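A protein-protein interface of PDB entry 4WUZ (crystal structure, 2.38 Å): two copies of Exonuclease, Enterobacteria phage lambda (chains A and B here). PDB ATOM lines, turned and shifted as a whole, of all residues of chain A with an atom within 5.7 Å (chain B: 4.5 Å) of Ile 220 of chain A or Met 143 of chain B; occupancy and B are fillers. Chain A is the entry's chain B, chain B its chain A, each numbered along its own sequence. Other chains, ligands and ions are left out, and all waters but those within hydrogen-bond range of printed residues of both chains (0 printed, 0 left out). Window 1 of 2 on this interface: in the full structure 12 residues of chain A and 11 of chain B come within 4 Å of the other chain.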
ATOM      1  N   HIS A  62      -7.585  19.026   7.377  1.00  0.00           N
ATOM      2  CA  HIS A  62      -6.110  18.962   7.348  1.00  0.00           C
ATOM      3  C   HIS A  62      -5.408  20.300   7.660  1.00  0.00           C
ATOM      4  O   HIS A  62      -4.298  20.330   8.181  1.00  0.00           O
ATOM      5  CB  HIS A  62      -5.675  18.438   5.956  1.00  0.00           C
ATOM      6  CG  HIS A  62      -5.874  16.966   5.784  1.00  0.00           C
ATOM      7  ND1 HIS A  62      -6.253  16.396   4.592  1.00  0.00           N
ATOM      8  CD2 HIS A  62      -5.795  15.955   6.679  1.00  0.00           C
ATOM      9  CE1 HIS A  62      -6.382  15.096   4.760  1.00  0.00           C
ATOM     10  NE2 HIS A  62      -6.090  14.805   6.015  1.00  0.00           N
ATOM     11  N   LEU A  65      -5.725  20.562  11.525  1.00  0.00           N
ATOM     12  CA  LEU A  65      -4.759  19.650  12.131  1.00  0.00           C
ATOM     13  C   LEU A  65      -3.334  20.212  12.049  1.00  0.00           C
ATOM     14  O   LEU A  65      -2.553  20.075  12.992  1.00  0.00           O
ATOM     15  CB  LEU A  65      -4.838  18.238  11.507  1.00  0.00           C
ATOM     16  CG  LEU A  65      -6.199  17.596  11.790  1.00  0.00           C
ATOM     17  CD1 LEU A  65      -6.437  16.384  10.976  1.00  0.00           C
ATOM     18  CD2 LEU A  65      -6.369  17.262  13.269  1.00  0.00           C
ATOM     19  N   ALA A  66      -3.000  20.828  10.929  1.00  0.00           N
ATOM     20  CA  ALA A  66      -1.678  21.458  10.735  1.00  0.00           C
ATOM     21  C   ALA A  66      -1.497  22.642  11.654  1.00  0.00           C
ATOM     22  O   ALA A  66      -0.383  22.917  12.114  1.00  0.00           O
ATOM     23  CB  ALA A  66      -1.518  21.917   9.305  1.00  0.00           C
ATOM     24  N   CYS A  69      -0.406  21.179  14.971  1.00  0.00           N
ATOM     25  CA  CYS A  69       0.904  20.528  15.072  1.00  0.00           C
ATOM     26  C   CYS A  69       2.067  21.443  14.684  1.00  0.00           C
ATOM     27  O   CYS A  69       3.190  21.089  14.942  1.00  0.00           O
ATOM     28  CB  CYS A  69       0.945  19.290  14.211  1.00  0.00           C
ATOM     29  SG  CYS A  69      -0.356  18.151  14.593  1.00  0.00           S
ATOM     30  N   GLU A 215      -9.078  11.960  16.756  1.00  0.00           N
ATOM     31  CA  GLU A 215      -8.613  10.654  16.287  1.00  0.00           C
ATOM     32  C   GLU A 215      -7.308  10.808  15.527  1.00  0.00           C
ATOM     33  O   GLU A 215      -6.287  10.227  15.892  1.00  0.00           O
ATOM     34  CB  GLU A 215      -9.649   9.996  15.363  1.00  0.00           C
ATOM     35  CG  GLU A 215     -10.650   9.078  16.042  1.00  0.00           C
ATOM     36  CD  GLU A 215     -11.657   8.517  15.044  1.00  0.00           C
ATOM     37  OE1 GLU A 215     -11.192   7.987  13.987  1.00  0.00           O
ATOM     38  OE2 GLU A 215     -12.894   8.654  15.317  1.00  0.00           O
ATOM     39  N   ALA A 216      -7.349  11.629  14.486  1.00  0.00           N
ATOM     40  CA  ALA A 216      -6.191  11.865  13.674  1.00  0.00           C
ATOM     41  C   ALA A 216      -4.966  12.391  14.462  1.00  0.00           C
ATOM     42  O   ALA A 216      -3.862  11.940  14.212  1.00  0.00           O
ATOM     43  CB  ALA A 216      -6.535  12.775  12.516  1.00  0.00           C
ATOM     44  N   LEU A 217      -5.138  13.319  15.411  1.00  0.00           N
ATOM     45  CA  LEU A 217      -3.966  13.824  16.172  1.00  0.00           C
ATOM     46  C   LEU A 217      -3.285  12.718  17.004  1.00  0.00           C
ATOM     47  O   LEU A 217      -2.054  12.573  16.968  1.00  0.00           O
ATOM     48  CB  LEU A 217      -4.315  15.033  17.064  1.00  0.00           C
ATOM     49  CG  LEU A 217      -4.775  16.379  16.480  1.00  0.00           C
ATOM     50  CD1 LEU A 217      -5.489  17.226  17.574  1.00  0.00           C
ATOM     51  CD2 LEU A 217      -3.622  17.161  15.881  1.00  0.00           C
ATOM     52  N   ALA A 218      -4.091  11.972  17.767  1.00  0.00           N
ATOM     53  CA  ALA A 218      -3.654  10.771  18.486  1.00  0.00           C
ATOM     54  C   ALA A 218      -2.800   9.862  17.594  1.00  0.00           C
ATOM     55  O   ALA A 218      -1.745   9.397  18.019  1.00  0.00           O
ATOM     56  CB  ALA A 218      -4.886   9.986  19.042  1.00  0.00           C
ATOM     57  N   GLU A 219      -3.251   9.632  16.361  1.00  0.00           N
ATOM     58  CA  GLU A 219      -2.579   8.718  15.481  1.00  0.00           C
ATOM     59  C   GLU A 219      -1.167   9.143  15.318  1.00  0.00           C
ATOM     60  O   GLU A 219      -0.269   8.302  15.321  1.00  0.00           O
ATOM     61  CB  GLU A 219      -3.231   8.654  14.112  1.00  0.00           C
ATOM     62  CG  GLU A 219      -4.392   7.708  14.008  1.00  0.00           C
ATOM     63  CD  GLU A 219      -4.929   7.628  12.583  1.00  0.00           C
ATOM     64  OE1 GLU A 219      -4.184   8.030  11.657  1.00  0.00           O
ATOM     65  OE2 GLU A 219      -6.087   7.145  12.384  1.00  0.00           O
ATOM     66  N   ILE A 220      -0.947  10.440  15.182  1.00  0.00           N
ATOM     67  CA  ILE A 220       0.381  10.891  14.952  1.00  0.00           C
ATOM     68  C   ILE A 220       1.030  11.480  16.181  1.00  0.00           C
ATOM     69  O   ILE A 220       2.100  12.048  16.070  1.00  0.00           O
ATOM     70  CB  ILE A 220       0.484  11.877  13.735  1.00  0.00           C
ATOM     71  CG1 ILE A 220       0.024  13.314  14.131  1.00  0.00           C
ATOM     72  CG2 ILE A 220      -0.192  11.268  12.553  1.00  0.00           C
ATOM     73  CD1 ILE A 220       0.025  14.332  13.001  1.00  0.00           C
ATOM     74  N   GLY A 221       0.400  11.335  17.349  1.00  0.00           N
ATOM     75  CA  GLY A 221       1.078  11.643  18.635  1.00  0.00           C
ATOM     76  C   GLY A 221       1.070  13.095  19.092  1.00  0.00           C
ATOM     77  O   GLY A 221       1.912  13.520  19.887  1.00  0.00           O
ATOM     78  N   PHE A 222       0.069  13.844  18.611  1.00  0.00           N
ATOM     79  CA  PHE A 222      -0.203  15.212  19.064  1.00  0.00           C
ATOM     80  C   PHE A 222      -1.474  15.276  19.868  1.00  0.00           C
ATOM     81  O   PHE A 222      -2.335  14.355  19.802  1.00  0.00           O
ATOM     82  CB  PHE A 222      -0.346  16.112  17.834  1.00  0.00           C
ATOM     83  CG  PHE A 222       0.961  16.580  17.281  1.00  0.00           C
ATOM     84  CD1 PHE A 222       1.612  15.841  16.330  1.00  0.00           C
ATOM     85  CD2 PHE A 222       1.534  17.767  17.721  1.00  0.00           C
ATOM     86  CE1 PHE A 222       2.791  16.250  15.820  1.00  0.00           C
ATOM     87  CE2 PHE A 222       2.751  18.186  17.215  1.00  0.00           C
ATOM     88  CZ  PHE A 222       3.390  17.424  16.269  1.00  0.00           C
ATOM     89  N   SER B 139       1.347  23.492   5.084  1.00  0.00           N
ATOM     90  CA  SER B 139       1.420  22.390   6.053  1.00  0.00           C
ATOM     91  C   SER B 139       0.175  21.532   5.940  1.00  0.00           C
ATOM     92  O   SER B 139       0.149  20.415   6.376  1.00  0.00           O
ATOM     93  CB  SER B 139       1.548  22.922   7.462  1.00  0.00           C
ATOM     94  OG  SER B 139       2.756  23.602   7.594  1.00  0.00           O
ATOM     95  N   ARG B 140      -0.850  22.080   5.327  1.00  0.00           N
ATOM     96  CA  ARG B 140      -2.067  21.353   5.005  1.00  0.00           C
ATOM     97  C   ARG B 140      -1.732  20.120   4.167  1.00  0.00           C
ATOM     98  O   ARG B 140      -2.259  19.030   4.432  1.00  0.00           O
ATOM     99  CB  ARG B 140      -3.012  22.265   4.212  1.00  0.00           C
ATOM    100  CG  ARG B 140      -4.334  21.597   3.863  1.00  0.00           C
ATOM    101  CD  ARG B 140      -5.045  22.255   2.684  1.00  0.00           C
ATOM    102  NE  ARG B 140      -4.254  22.040   1.494  1.00  0.00           N
ATOM    103  CZ  ARG B 140      -4.003  23.006   0.641  1.00  0.00           C
ATOM    104  NH1 ARG B 140      -4.530  24.196   0.859  1.00  0.00           N
ATOM    105  NH2 ARG B 140      -3.243  22.787  -0.416  1.00  0.00           N
ATOM    106  N   ASP B 141      -0.862  20.288   3.158  1.00  0.00           N
ATOM    107  CA  ASP B 141      -0.542  19.189   2.287  1.00  0.00           C
ATOM    108  C   ASP B 141       0.370  18.205   3.025  1.00  0.00           C
ATOM    109  O   ASP B 141       0.201  16.997   2.898  1.00  0.00           O
ATOM    110  CB  ASP B 141       0.080  19.645   0.976  1.00  0.00           C
ATOM    111  CG  ASP B 141      -0.939  20.278   0.004  1.00  0.00           C
ATOM    112  OD1 ASP B 141      -2.142  19.949   0.036  1.00  0.00           O
ATOM    113  OD2 ASP B 141      -0.510  21.102  -0.824  1.00  0.00           O
ATOM    114  N   PHE B 142       1.300  18.702   3.837  1.00  0.00           N
ATOM    115  CA  PHE B 142       2.133  17.779   4.574  1.00  0.00           C
ATOM    116  C   PHE B 142       1.197  16.828   5.299  1.00  0.00           C
ATOM    117  O   PHE B 142       1.349  15.635   5.208  1.00  0.00           O
ATOM    118  CB  PHE B 142       3.024  18.452   5.604  1.00  0.00           C
ATOM    119  CG  PHE B 142       3.856  17.473   6.369  1.00  0.00           C
ATOM    120  CD1 PHE B 142       3.526  17.128   7.683  1.00  0.00           C
ATOM    121  CD2 PHE B 142       4.918  16.810   5.736  1.00  0.00           C
ATOM    122  CE1 PHE B 142       4.273  16.200   8.369  1.00  0.00           C
ATOM    123  CE2 PHE B 142       5.690  15.873   6.429  1.00  0.00           C
ATOM    124  CZ  PHE B 142       5.372  15.567   7.747  1.00  0.00           C
ATOM    125  N   MET B 143       0.201  17.402   5.963  1.00  0.00           N
ATOM    126  CA  MET B 143      -0.665  16.705   6.900  1.00  0.00           C
ATOM    127  C   MET B 143      -1.476  15.680   6.162  1.00  0.00           C
ATOM    128  O   MET B 143      -1.643  14.579   6.634  1.00  0.00           O
ATOM    129  CB  MET B 143      -1.625  17.689   7.589  1.00  0.00           C
ATOM    130  CG  MET B 143      -1.411  17.969   9.074  1.00  0.00           C
ATOM    131  SD  MET B 143      -1.201  16.609  10.293  1.00  0.00           S
ATOM    132  CE  MET B 143      -2.427  15.447   9.793  1.00  0.00           C
ATOM    133  N   LYS B 144      -1.975  16.056   5.001  1.00  0.00           N
ATOM    134  CA  LYS B 144      -2.780  15.177   4.191  1.00  0.00           C
ATOM    135  C   LYS B 144      -2.020  13.848   3.932  1.00  0.00           C
ATOM    136  O   LYS B 144      -2.566  12.743   4.049  1.00  0.00           O
ATOM    137  CB  LYS B 144      -3.099  15.894   2.885  1.00  0.00           C
ATOM    138  CG  LYS B 144      -4.144  15.198   2.065  1.00  0.00           C
ATOM    139  CD  LYS B 144      -4.081  15.542   0.579  1.00  0.00           C
ATOM    140  CE  LYS B 144      -4.993  14.548  -0.220  1.00  0.00           C
ATOM    141  NZ  LYS B 144      -5.096  14.863  -1.697  1.00  0.00           N
ATOM    142  N   PHE B 145      -0.744  13.966   3.605  1.00  0.00           N
ATOM    143  CA  PHE B 145       0.018  12.800   3.247  1.00  0.00           C
ATOM    144  C   PHE B 145       0.460  12.045   4.516  1.00  0.00           C
ATOM    145  O   PHE B 145       0.437  10.826   4.546  1.00  0.00           O
ATOM    146  CB  PHE B 145       1.168  13.209   2.331  1.00  0.00           C
ATOM    147  CG  PHE B 145       2.228  12.162   2.165  1.00  0.00           C
ATOM    148  CD1 PHE B 145       1.917  10.897   1.668  1.00  0.00           C
ATOM    149  CD2 PHE B 145       3.557  12.465   2.462  1.00  0.00           C
ATOM    150  CE1 PHE B 145       2.920   9.954   1.509  1.00  0.00           C
ATOM    151  CE2 PHE B 145       4.574  11.532   2.299  1.00  0.00           C
ATOM    152  CZ  PHE B 145       4.259  10.277   1.842  1.00  0.00           C
ATOM    153  N   ARG B 146       0.797  12.770   5.575  1.00  0.00           N
ATOM    154  CA  ARG B 146       1.145  12.156   6.836  1.00  0.00           C
ATOM    155  C   ARG B 146       0.090  11.196   7.466  1.00  0.00           C
ATOM    156  O   ARG B 146       0.446  10.350   8.293  1.00  0.00           O
ATOM    157  CB  ARG B 146       1.504  13.236   7.837  1.00  0.00           C
ATOM    158  CG  ARG B 146       1.881  12.673   9.176  1.00  0.00           C
ATOM    159  CD  ARG B 146       3.108  11.803   9.074  1.00  0.00           C
ATOM    160  NE  ARG B 146       3.469  11.263  10.372  1.00  0.00           N
ATOM    161  CZ  ARG B 146       2.922  10.175  10.926  1.00  0.00           C
ATOM    162  NH1 ARG B 146       1.921   9.473  10.328  1.00  0.00           N
ATOM    163  NH2 ARG B 146       3.379   9.808  12.097  1.00  0.00           N
ATOM    164  N   LEU B 147      -1.171  11.323   7.078  1.00  0.00           N
ATOM    165  CA  LEU B 147      -2.244  10.609   7.718  1.00  0.00           C
ATOM    166  C   LEU B 147      -2.820   9.579   6.772  1.00  0.00           C
ATOM    167  O   LEU B 147      -3.128   8.462   7.174  1.00  0.00           O
ATOM    168  CB  LEU B 147      -3.384  11.584   8.113  1.00  0.00           C
ATOM    169  CG  LEU B 147      -3.257  12.531   9.307  1.00  0.00           C
ATOM    170  CD1 LEU B 147      -4.521  13.408   9.387  1.00  0.00           C
ATOM    171  CD2 LEU B 147      -3.014  11.813  10.644  1.00  0.00           C
ATOM    172  N   GLU B 185       8.546  15.471  14.092  1.00  0.00           N
ATOM    173  CA  GLU B 185       8.136  14.502  13.044  1.00  0.00           C
ATOM    174  C   GLU B 185       7.648  15.103  11.714  1.00  0.00           C
ATOM    175  O   GLU B 185       6.604  14.692  11.172  1.00  0.00           O
ATOM    176  CB  GLU B 185       7.075  13.564  13.549  1.00  0.00           C
ATOM    177  CG  GLU B 185       7.571  12.515  14.523  1.00  0.00           C
ATOM    178  CD  GLU B 185       6.404  11.886  15.237  1.00  0.00           C
ATOM    179  OE1 GLU B 185       6.494  11.744  16.484  1.00  0.00           O
ATOM    180  OE2 GLU B 185       5.380  11.595  14.544  1.00  0.00           O
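Printed residues of chain B within 4 Å of Leu 65 of chain A: Leu 147 (3.9 Å). Printed residues of chain B within 4 Å of Ala 66 of chain A: Ser 139 (3.7 Å) and Met 143 (3.8 Å). Of chain B, only Met 143 (3.7 Å), Arg 146 (3.6 Å), Leu 147 (3.5 Å) and Glu 185 (3.6 Å) come within 4 Å of Ile 220 of chain A. Of chain A, only His 62 (3.8 Å), Ala 66 (3.8 Å) and Ile 220 (3.7 Å) come within 4 Å of Met 143 of chain B. Of the printed residues of chain A, Arg 146 of chain B touches Ile 220 (3.6 Å). Of the printed residues of chain A, Leu 147 of chain B touches His 62 (3.9 Å), Leu 65 (3.9 Å), Ala 216 (3.7 Å) and Ile 220 (3.5 Å).
The guanidinium group (NH2) of Arg 146 of chain B lies within salt-bridge range of the side-chain carboxylate (OE2) of Glu 185 of chain B (3.6 Å). SG of Cys 69 of chain A sits at hydrogen-bond distance from O of Leu 65 of chain A (3.3 Å). The side-chain carboxylate of Asp 141 of chain B lies within salt-bridge range of the guanidinium group of Arg 140 of chain B (3.1 Å).
No position is printed for both chains.
O of Arg 140 of chain B touches CB of His 62 of chain A, at 3.8 Å. His 62 of chain A touches Met 143 of chain B (O to CB, 3.8 Å). CD1 of Leu 147 of chain B touches CD2 of His 62 of chain A, 3.9 Å away. CD1 of Leu 65 of chain A touches CD1 of Leu 147 of chain B (3.9 Å). Ala 66 of chain A touches Ser 139 of chain B (CB to O, 3.7 Å). CG of Met 143 of chain B touches N of Ala 66 of chain A, 3.8 Å away. Ala 216 of chain A touches Leu 147 of chain B. Ile 220 of chain A touches Arg 146 of chain B (CG2 to NH1, 3.6 Å). CG2 of Ile 220 of chain A touches CD2 of Leu 147 of chain B, at 3.5 Å. Ile 220 of chain A touches Glu 185 of chain B (O to OE2, 3.6 Å).
Of the 10 printed residues of chain B, 7 touch a printed residue of chain A. Hydrophobic or aromatic side chains of chain A within 4 Å of the printed part of chain B: His 62, Leu 65, Ala 66, Ala 216 and Ile 220. Among the printed residues, no Asp or Glu carboxylate lies within 4 Å of a Lys or Arg side-chain nitrogen of the other chain.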
